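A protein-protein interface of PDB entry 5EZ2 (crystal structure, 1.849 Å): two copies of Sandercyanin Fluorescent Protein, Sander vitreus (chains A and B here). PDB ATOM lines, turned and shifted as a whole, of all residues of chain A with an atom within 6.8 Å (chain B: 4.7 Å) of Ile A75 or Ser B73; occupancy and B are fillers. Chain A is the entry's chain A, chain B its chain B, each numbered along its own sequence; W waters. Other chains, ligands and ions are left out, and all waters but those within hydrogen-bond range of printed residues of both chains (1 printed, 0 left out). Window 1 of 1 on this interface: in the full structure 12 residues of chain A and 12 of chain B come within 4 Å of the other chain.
The backbone carbonyl oxygen (O) of Ser B73 lies within hydrogen-bond range of the backbone NH (N) of Phe B88, 2.8 Å away. The backbone NH (N) of Val B56 lies within hydrogen-bond range of the backbone carbonyl oxygen (O) of Gly B72 (2.8 Å). N of Phe A88 is in hydrogen-bond range of O of Ser A73 (2.8 Å). The backbone NH (N) of Gln B86 sits at hydrogen-bond distance from the backbone carbonyl oxygen (O) of Ile B75 (2.8 Å). The backbone NH of Gln A86 is in hydrogen-bond range of the backbone carbonyl oxygen of Ile A75, 2.7 Å away. The side-chain hydroxyl of Ser A49 lies within hydrogen-bond range of the backbone carbonyl oxygen of Val A52, at 3.5 Å.
Hydrophobic or aromatic side chains of chain A within 4 Å of the printed part of chain B: Pro A50, Val A52, Ile A75 and Phe A88. Among the printed residues, 13 pairs touch across the chains. Among the printed residues, no Asp or Glu carboxylate lies within 4 Å of a Lys or Arg side-chain nitrogen of the other chain.
Printed residues of chain B within 4 Å of Val A52: Gly B72 (3.9 Å), Ser B73 (2.8 Å) and Phe B88 (3.3 Å). Ala A74 touches none of the printed residues of chain B. Of chain B, only Ser B73 (3.9 Å), Ile B75 (3.95 Å) and Phe B88 (3.5 Å) come within 4 Å of Ile A75. Leu A85 touches none of the printed residues of chain B. Ser B73 touches just these residues of chain A: Gly A51 (3.4 Å), Val A52 (2.8 Å) and Ile A75 (3.9 Å). Of the printed residues of chain A, Ile B75 touches Ile A75 and Phe A88. The nearest residue of chain A that does not touch Ser B73 is Ser A49 (5.0 Å). The nearest printed residue of chain A that does not touch Gly B72 is Pro A50 (5.1 Å).
Water W1 lies within hydrogen-bond range of O of Val B56 (2.8 Å) and O of Pro A50 (3.0 Å).
Ile A75 touches Ser B73, but with the chains exchanged Ser A73 does not touch Ile B75 (4.02 Å). Ile A75 touches its own counterpart, Ile B75. Ile A75 touches Phe B88, and with the chains exchanged Phe A88 touches Ile B75. Phe A88 touches its own counterpart, Phe B88. Positions printed for both chains: 54, 73, 74, 75, 86, 87 and 88. Of the 13 pairs that touch across the chains among the printed residues, 4 have their exchanged pair printed and touching as well.
OG of Ser B73 lies within hydrogen-bond range of N of Val A52.
CB of Pro A50 touches OG of Ser B55, at 3.8 Å. N of Gly A51 touches CB of Ser B55, 3.8 Å away. Gly B72 touches Gly A51 (O to CA, 3.3 Å). Ser B73 touches Gly A51 (OG to CA, 3.4 Å). Val A52 touches Phe B88 (CG2 to O, 3.3 Å). Ile A75 touches Ser B73. Ile B75 touches Ile A75 (CD1 to CD1, 3.95 Å). CD1 of Phe B88 touches CD1 of Ile A75, at 3.5 Å. Phe B88 touches Glu A77 (CE2 to OE2, 3.7 Å). Phe A88 touches Ile B75 (CD1 to CD1, 3.6 Å).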
ATOM      1  N   SER A  49      -1.437  -9.111   5.007  1.00  0.00           N
ATOM      2  CA  SER A  49       0.008  -9.197   4.843  1.00  0.00           C
ATOM      3  C   SER A  49       0.330  -9.628   3.421  1.00  0.00           C
ATOM      4  O   SER A  49      -0.465 -10.325   2.785  1.00  0.00           O
ATOM      5  CB  SER A  49       0.634 -10.150   5.863  1.00  0.00           C
ATOM      6  OG  SER A  49       0.297 -11.500   5.600  1.00  0.00           O
ATOM      7  N   PRO A  50       1.495  -9.196   2.913  1.00  0.00           N
ATOM      8  CA  PRO A  50       1.941  -9.522   1.557  1.00  0.00           C
ATOM      9  C   PRO A  50       2.197 -11.020   1.435  1.00  0.00           C
ATOM     10  O   PRO A  50       2.077 -11.578   0.341  1.00  0.00           O
ATOM     11  CB  PRO A  50       3.269  -8.759   1.424  1.00  0.00           C
ATOM     12  CG  PRO A  50       3.288  -7.777   2.539  1.00  0.00           C
ATOM     13  CD  PRO A  50       2.496  -8.408   3.647  1.00  0.00           C
ATOM     14  N   GLY A  51       2.537 -11.663   2.548  1.00  0.00           N
ATOM     15  CA  GLY A  51       2.795 -13.095   2.540  1.00  0.00           C
ATOM     16  C   GLY A  51       1.534 -13.889   2.805  1.00  0.00           C
ATOM     17  O   GLY A  51       0.441 -13.429   2.496  1.00  0.00           O
ATOM     18  N   VAL A  52       1.673 -15.082   3.376  1.00  0.00           N
ATOM     19  CA  VAL A  52       0.504 -15.888   3.709  1.00  0.00           C
ATOM     20  C   VAL A  52       0.001 -15.501   5.094  1.00  0.00           C
ATOM     21  O   VAL A  52       0.753 -14.937   5.891  1.00  0.00           O
ATOM     22  CB  VAL A  52       0.802 -17.410   3.675  1.00  0.00           C
ATOM     23  CG1 VAL A  52       1.264 -17.843   2.289  1.00  0.00           C
ATOM     24  CG2 VAL A  52       1.825 -17.787   4.732  1.00  0.00           C
ATOM     25  N   GLY A  53      -1.260 -15.796   5.383  1.00  0.00           N
ATOM     26  CA  GLY A  53      -1.810 -15.497   6.696  1.00  0.00           C
ATOM     27  C   GLY A  53      -2.046 -14.008   6.868  1.00  0.00           C
ATOM     28  O   GLY A  53      -2.197 -13.280   5.879  1.00  0.00           O
ATOM     29  N   PHE A  54      -2.075 -13.542   8.115  1.00  0.00           N
ATOM     30  CA  PHE A  54      -2.322 -12.121   8.368  1.00  0.00           C
ATOM     31  C   PHE A  54      -1.445 -11.588   9.492  1.00  0.00           C
ATOM     32  O   PHE A  54      -0.822 -12.362  10.235  1.00  0.00           O
ATOM     33  CB  PHE A  54      -3.820 -11.832   8.618  1.00  0.00           C
ATOM     34  CG  PHE A  54      -4.442 -12.660   9.712  1.00  0.00           C
ATOM     35  CD1 PHE A  54      -4.442 -12.217  11.029  1.00  0.00           C
ATOM     36  CD2 PHE A  54      -5.037 -13.880   9.421  1.00  0.00           C
ATOM     37  CE1 PHE A  54      -5.026 -12.980  12.037  1.00  0.00           C
ATOM     38  CE2 PHE A  54      -5.624 -14.642  10.412  1.00  0.00           C
ATOM     39  CZ  PHE A  54      -5.615 -14.195  11.727  1.00  0.00           C
ATOM     40  N   SER A  73       2.439 -12.509  13.655  1.00  0.00           N
ATOM     41  CA  SER A  73       1.945 -12.985  12.373  1.00  0.00           C
ATOM     42  C   SER A  73       1.112 -14.202  12.674  1.00  0.00           C
ATOM     43  O   SER A  73       1.459 -14.983  13.571  1.00  0.00           O
ATOM     44  CB  SER A  73       3.109 -13.397  11.468  1.00  0.00           C
ATOM     45  OG  SER A  73       3.869 -12.274  11.081  1.00  0.00           O
ATOM     46  N   ALA A  74       0.026 -14.366  11.921  1.00  0.00           N
ATOM     47  CA  ALA A  74      -0.876 -15.494  12.094  1.00  0.00           C
ATOM     48  C   ALA A  74      -0.844 -16.306  10.814  1.00  0.00           C
ATOM     49  O   ALA A  74      -0.966 -15.743   9.720  1.00  0.00           O
ATOM     50  CB  ALA A  74      -2.290 -15.004  12.360  1.00  0.00           C
ATOM     51  N   ILE A  75      -0.703 -17.623  10.947  1.00  0.00           N
ATOM     52  CA  ILE A  75      -0.668 -18.496   9.773  1.00  0.00           C
ATOM     53  C   ILE A  75      -1.394 -19.799  10.075  1.00  0.00           C
ATOM     54  O   ILE A  75      -1.210 -20.392  11.147  1.00  0.00           O
ATOM     55  CB  ILE A  75       0.778 -18.824   9.383  1.00  0.00           C
ATOM     56  CG1 ILE A  75       1.501 -17.565   8.886  1.00  0.00           C
ATOM     57  CG2 ILE A  75       0.826 -19.940   8.309  1.00  0.00           C
ATOM     58  CD1 ILE A  75       2.961 -17.800   8.573  1.00  0.00           C
ATOM     59  N   ALA A  76      -2.220 -20.249   9.134  1.00  0.00           N
ATOM     60  CA  ALA A  76      -2.822 -21.573   9.243  1.00  0.00           C
ATOM     61  C   ALA A  76      -1.895 -22.566   8.556  1.00  0.00           C
ATOM     62  O   ALA A  76      -1.822 -22.611   7.322  1.00  0.00           O
ATOM     63  CB  ALA A  76      -4.197 -21.593   8.602  1.00  0.00           C
ATOM     64  N   GLU A  77      -1.172 -23.349   9.345  1.00  0.00           N
ATOM     65  CA  GLU A  77      -0.146 -24.231   8.783  1.00  0.00           C
ATOM     66  C   GLU A  77      -0.734 -25.332   7.908  1.00  0.00           C
ATOM     67  O   GLU A  77      -0.068 -25.823   6.984  1.00  0.00           O
ATOM     68  CB  GLU A  77       0.747 -24.798   9.885  1.00  0.00           C
ATOM     69  CG  GLU A  77       1.542 -23.695  10.606  1.00  0.00           C
ATOM     70  CD  GLU A  77       2.534 -24.234  11.618  1.00  0.00           C
ATOM     71  OE1 GLU A  77       2.653 -25.467  11.738  1.00  0.00           O
ATOM     72  OE2 GLU A  77       3.198 -23.420  12.302  1.00  0.00           O
ATOM     73  N   ASP A  78      -1.975 -25.714   8.198  1.00  0.00           N
ATOM     74  CA  ASP A  78      -2.711 -26.635   7.333  1.00  0.00           C
ATOM     75  C   ASP A  78      -3.816 -25.870   6.629  1.00  0.00           C
ATOM     76  O   ASP A  78      -4.849 -25.561   7.235  1.00  0.00           O
ATOM     77  CB  ASP A  78      -3.321 -27.776   8.143  1.00  0.00           C
ATOM     78  CG  ASP A  78      -4.090 -28.763   7.274  1.00  0.00           C
ATOM     79  OD1 ASP A  78      -4.286 -28.492   6.065  1.00  0.00           O
ATOM     80  OD2 ASP A  78      -4.520 -29.806   7.810  1.00  0.00           O
ATOM     81  N   PRO A  82      -8.352 -23.780   8.092  1.00  0.00           N
ATOM     82  CA  PRO A  82      -7.990 -22.358   8.162  1.00  0.00           C
ATOM     83  C   PRO A  82      -8.279 -21.713   9.520  1.00  0.00           C
ATOM     84  O   PRO A  82      -7.709 -20.654   9.804  1.00  0.00           O
ATOM     85  CB  PRO A  82      -8.861 -21.711   7.066  1.00  0.00           C
ATOM     86  CG  PRO A  82     -10.017 -22.649   6.890  1.00  0.00           C
ATOM     87  CD  PRO A  82      -9.433 -24.030   7.123  1.00  0.00           C
ATOM     88  N   LYS A  84      -7.542 -23.086  12.382  1.00  0.00           N
ATOM     89  CA  LYS A  84      -6.569 -23.559  13.364  1.00  0.00           C
ATOM     90  C   LYS A  84      -5.249 -22.908  13.038  1.00  0.00           C
ATOM     91  O   LYS A  84      -4.488 -23.401  12.210  1.00  0.00           O
ATOM     92  CB  LYS A  84      -6.454 -25.084  13.344  1.00  0.00           C
ATOM     93  CG  LYS A  84      -7.741 -25.777  13.764  1.00  0.00           C
ATOM     94  CD  LYS A  84      -7.557 -27.295  13.815  1.00  0.00           C
ATOM     95  CE  LYS A  84      -8.760 -27.950  14.491  1.00  0.00           C
ATOM     96  NZ  LYS A  84      -8.660 -29.439  14.458  1.00  0.00           N
ATOM     97  N   LEU A  85      -4.991 -21.784  13.694  1.00  0.00           N
ATOM     98  CA  LEU A  85      -3.874 -20.928  13.338  1.00  0.00           C
ATOM     99  C   LEU A  85      -2.717 -21.081  14.312  1.00  0.00           C
ATOM    100  O   LEU A  85      -2.894 -21.565  15.433  1.00  0.00           O
ATOM    101  CB  LEU A  85      -4.351 -19.478  13.324  1.00  0.00           C
ATOM    102  CG  LEU A  85      -5.458 -19.245  12.286  1.00  0.00           C
ATOM    103  CD1 LEU A  85      -6.560 -18.390  12.861  1.00  0.00           C
ATOM    104  CD2 LEU A  85      -4.883 -18.586  11.050  1.00  0.00           C
ATOM    105  N   GLN A  86      -1.531 -20.688  13.860  1.00  0.00           N
ATOM    106  CA  GLN A  86      -0.371 -20.560  14.722  1.00  0.00           C
ATOM    107  C   GLN A  86      -0.061 -19.070  14.764  1.00  0.00           C
ATOM    108  O   GLN A  86       0.014 -18.418  13.708  1.00  0.00           O
ATOM    109  CB  GLN A  86       0.803 -21.338  14.123  1.00  0.00           C
ATOM    110  CG  GLN A  86       1.829 -21.800  15.132  1.00  0.00           C
ATOM    111  CD  GLN A  86       1.309 -22.918  16.010  1.00  0.00           C
ATOM    112  OE1 GLN A  86       0.232 -23.476  15.770  1.00  0.00           O
ATOM    113  NE2 GLN A  86       2.060 -23.248  17.030  1.00  0.00           N
ATOM    114  N   PHE A  87       0.085 -18.516  15.968  1.00  0.00           N
ATOM    115  CA  PHE A  87       0.404 -17.094  16.118  1.00  0.00           C
ATOM    116  C   PHE A  87       1.862 -16.970  16.530  1.00  0.00           C
ATOM    117  O   PHE A  87       2.318 -17.639  17.471  1.00  0.00           O
ATOM    118  CB  PHE A  87      -0.486 -16.432  17.186  1.00  0.00           C
ATOM    119  CG  PHE A  87      -1.761 -15.822  16.644  1.00  0.00           C
ATOM    120  CD1 PHE A  87      -2.573 -16.526  15.762  1.00  0.00           C
ATOM    121  CD2 PHE A  87      -2.164 -14.557  17.054  1.00  0.00           C
ATOM    122  CE1 PHE A  87      -3.762 -15.967  15.271  1.00  0.00           C
ATOM    123  CE2 PHE A  87      -3.354 -13.984  16.572  1.00  0.00           C
ATOM    124  CZ  PHE A  87      -4.156 -14.696  15.680  1.00  0.00           C
ATOM    125  N   PHE A  88       2.594 -16.128  15.813  1.00  0.00           N
ATOM    126  CA  PHE A  88       4.000 -15.897  16.104  1.00  0.00           C
ATOM    127  C   PHE A  88       4.153 -14.457  16.566  1.00  0.00           C
ATOM    128  O   PHE A  88       4.158 -13.538  15.748  1.00  0.00           O
ATOM    129  CB  PHE A  88       4.840 -16.134  14.847  1.00  0.00           C
ATOM    130  CG  PHE A  88       4.643 -17.501  14.236  1.00  0.00           C
ATOM    131  CD1 PHE A  88       3.604 -17.732  13.346  1.00  0.00           C
ATOM    132  CD2 PHE A  88       5.495 -18.546  14.553  1.00  0.00           C
ATOM    133  CE1 PHE A  88       3.422 -18.983  12.775  1.00  0.00           C
ATOM    134  CE2 PHE A  88       5.325 -19.813  13.974  1.00  0.00           C
ATOM    135  CZ  PHE A  88       4.280 -20.026  13.097  1.00  0.00           C
ATOM    136  N   PHE B  54       9.524 -12.121   7.436  1.00  0.00           N
ATOM    137  CA  PHE B  54       9.500 -11.367   6.187  1.00  0.00           C
ATOM    138  C   PHE B  54       8.623 -12.079   5.160  1.00  0.00           C
ATOM    139  O   PHE B  54       8.221 -13.234   5.367  1.00  0.00           O
ATOM    140  CB  PHE B  54      10.921 -11.047   5.658  1.00  0.00           C
ATOM    141  CG  PHE B  54      11.827 -12.250   5.481  1.00  0.00           C
ATOM    142  CD1 PHE B  54      11.878 -12.935   4.269  1.00  0.00           C
ATOM    143  CD2 PHE B  54      12.671 -12.654   6.510  1.00  0.00           C
ATOM    144  CE1 PHE B  54      12.720 -14.031   4.106  1.00  0.00           C
ATOM    145  CE2 PHE B  54      13.523 -13.747   6.360  1.00  0.00           C
ATOM    146  CZ  PHE B  54      13.553 -14.434   5.151  1.00  0.00           C
ATOM    147  N   SER B  55       8.282 -11.389   4.078  1.00  0.00           N
ATOM    148  CA  SER B  55       7.378 -11.982   3.104  1.00  0.00           C
ATOM    149  C   SER B  55       8.177 -12.484   1.904  1.00  0.00           C
ATOM    150  O   SER B  55       9.301 -12.020   1.654  1.00  0.00           O
ATOM    151  CB  SER B  55       6.271 -11.004   2.695  1.00  0.00           C
ATOM    152  OG  SER B  55       6.814  -9.867   2.060  1.00  0.00           O
ATOM    153  N   VAL B  56       7.609 -13.452   1.191  1.00  0.00           N
ATOM    154  CA  VAL B  56       8.339 -14.186   0.155  1.00  0.00           C
ATOM    155  C   VAL B  56       7.556 -14.116  -1.149  1.00  0.00           C
ATOM    156  O   VAL B  56       6.334 -14.292  -1.160  1.00  0.00           O
ATOM    157  CB  VAL B  56       8.479 -15.676   0.538  1.00  0.00           C
ATOM    158  CG1 VAL B  56       9.157 -16.472  -0.594  1.00  0.00           C
ATOM    159  CG2 VAL B  56       9.255 -15.831   1.858  1.00  0.00           C
ATOM    160  N   GLY B  72       4.657 -16.336   0.017  1.00  0.00           N
ATOM    161  CA  GLY B  72       4.902 -17.073   1.240  1.00  0.00           C
ATOM    162  C   GLY B  72       5.300 -16.144   2.364  1.00  0.00           C
ATOM    163  O   GLY B  72       5.452 -14.929   2.157  1.00  0.00           O
ATOM    164  N   SER B  73       5.435 -16.712   3.554  1.00  0.00           N
ATOM    165  CA  SER B  73       5.945 -15.979   4.708  1.00  0.00           C
ATOM    166  C   SER B  73       7.109 -16.744   5.307  1.00  0.00           C
ATOM    167  O   SER B  73       7.107 -17.979   5.315  1.00  0.00           O
ATOM    168  CB  SER B  73       4.845 -15.797   5.753  1.00  0.00           C
ATOM    169  OG  SER B  73       3.812 -14.977   5.242  1.00  0.00           O
ATOM    170  N   ALA B  74       8.107 -16.007   5.788  1.00  0.00           N
ATOM    171  CA  ALA B  74       9.291 -16.592   6.394  1.00  0.00           C
ATOM    172  C   ALA B  74       9.351 -16.155   7.851  1.00  0.00           C
ATOM    173  O   ALA B  74       9.234 -14.962   8.146  1.00  0.00           O
ATOM    174  CB  ALA B  74      10.538 -16.125   5.661  1.00  0.00           C
ATOM    175  N   ILE B  75       9.524 -17.113   8.754  1.00  0.00           N
ATOM    176  CA  ILE B  75       9.628 -16.803  10.185  1.00  0.00           C
ATOM    177  C   ILE B  75      10.688 -17.660  10.847  1.00  0.00           C
ATOM    178  O   ILE B  75      10.739 -18.874  10.636  1.00  0.00           O
ATOM    179  CB  ILE B  75       8.275 -17.029  10.909  1.00  0.00           C
ATOM    180  CG1 ILE B  75       7.180 -16.176  10.249  1.00  0.00           C
ATOM    181  CG2 ILE B  75       8.399 -16.739  12.431  1.00  0.00           C
ATOM    182  CD1 ILE B  75       5.813 -16.315  10.871  1.00  0.00           C
ATOM    183  N   GLN B  86      11.390 -21.070   9.061  1.00  0.00           N
ATOM    184  CA  GLN B  86      10.315 -21.862   8.499  1.00  0.00           C
ATOM    185  C   GLN B  86       9.663 -21.022   7.413  1.00  0.00           C
ATOM    186  O   GLN B  86       9.332 -19.841   7.634  1.00  0.00           O
ATOM    187  CB  GLN B  86       9.312 -22.223   9.594  1.00  0.00           C
ATOM    188  CG  GLN B  86       9.843 -23.295  10.539  1.00  0.00           C
ATOM    189  CD  GLN B  86       9.878 -24.663   9.878  1.00  0.00           C
ATOM    190  OE1 GLN B  86       8.868 -25.141   9.363  1.00  0.00           O
ATOM    191  NE2 GLN B  86      11.046 -25.293   9.880  1.00  0.00           N
ATOM    192  N   PHE B  87       9.514 -21.610   6.226  1.00  0.00           N
ATOM    193  CA  PHE B  87       8.842 -20.930   5.122  1.00  0.00           C
ATOM    194  C   PHE B  87       7.457 -21.517   4.926  1.00  0.00           C
ATOM    195  O   PHE B  87       7.291 -22.741   4.839  1.00  0.00           O
ATOM    196  CB  PHE B  87       9.630 -21.079   3.811  1.00  0.00           C
ATOM    197  CG  PHE B  87      10.653 -20.002   3.575  1.00  0.00           C
ATOM    198  CD1 PHE B  87      11.479 -19.555   4.608  1.00  0.00           C
ATOM    199  CD2 PHE B  87      10.818 -19.458   2.302  1.00  0.00           C
ATOM    200  CE1 PHE B  87      12.436 -18.568   4.370  1.00  0.00           C
ATOM    201  CE2 PHE B  87      11.777 -18.479   2.053  1.00  0.00           C
ATOM    202  CZ  PHE B  87      12.590 -18.037   3.083  1.00  0.00           C
ATOM    203  N   PHE B  88       6.470 -20.633   4.833  1.00  0.00           N
ATOM    204  CA  PHE B  88       5.086 -21.041   4.682  1.00  0.00           C
ATOM    205  C   PHE B  88       4.613 -20.537   3.340  1.00  0.00           C
ATOM    206  O   PHE B  88       4.342 -19.345   3.195  1.00  0.00           O
ATOM    207  CB  PHE B  88       4.231 -20.435   5.802  1.00  0.00           C
ATOM    208  CG  PHE B  88       4.718 -20.774   7.187  1.00  0.00           C
ATOM    209  CD1 PHE B  88       5.655 -19.971   7.822  1.00  0.00           C
ATOM    210  CD2 PHE B  88       4.240 -21.895   7.853  1.00  0.00           C
ATOM    211  CE1 PHE B  88       6.109 -20.278   9.110  1.00  0.00           C
ATOM    212  CE2 PHE B  88       4.688 -22.208   9.136  1.00  0.00           C
ATOM    213  CZ  PHE B  88       5.625 -21.397   9.761  1.00  0.00           C
HETATM  214  O   HOH W   1       4.769 -12.003  -0.863  1.00  0.00           O
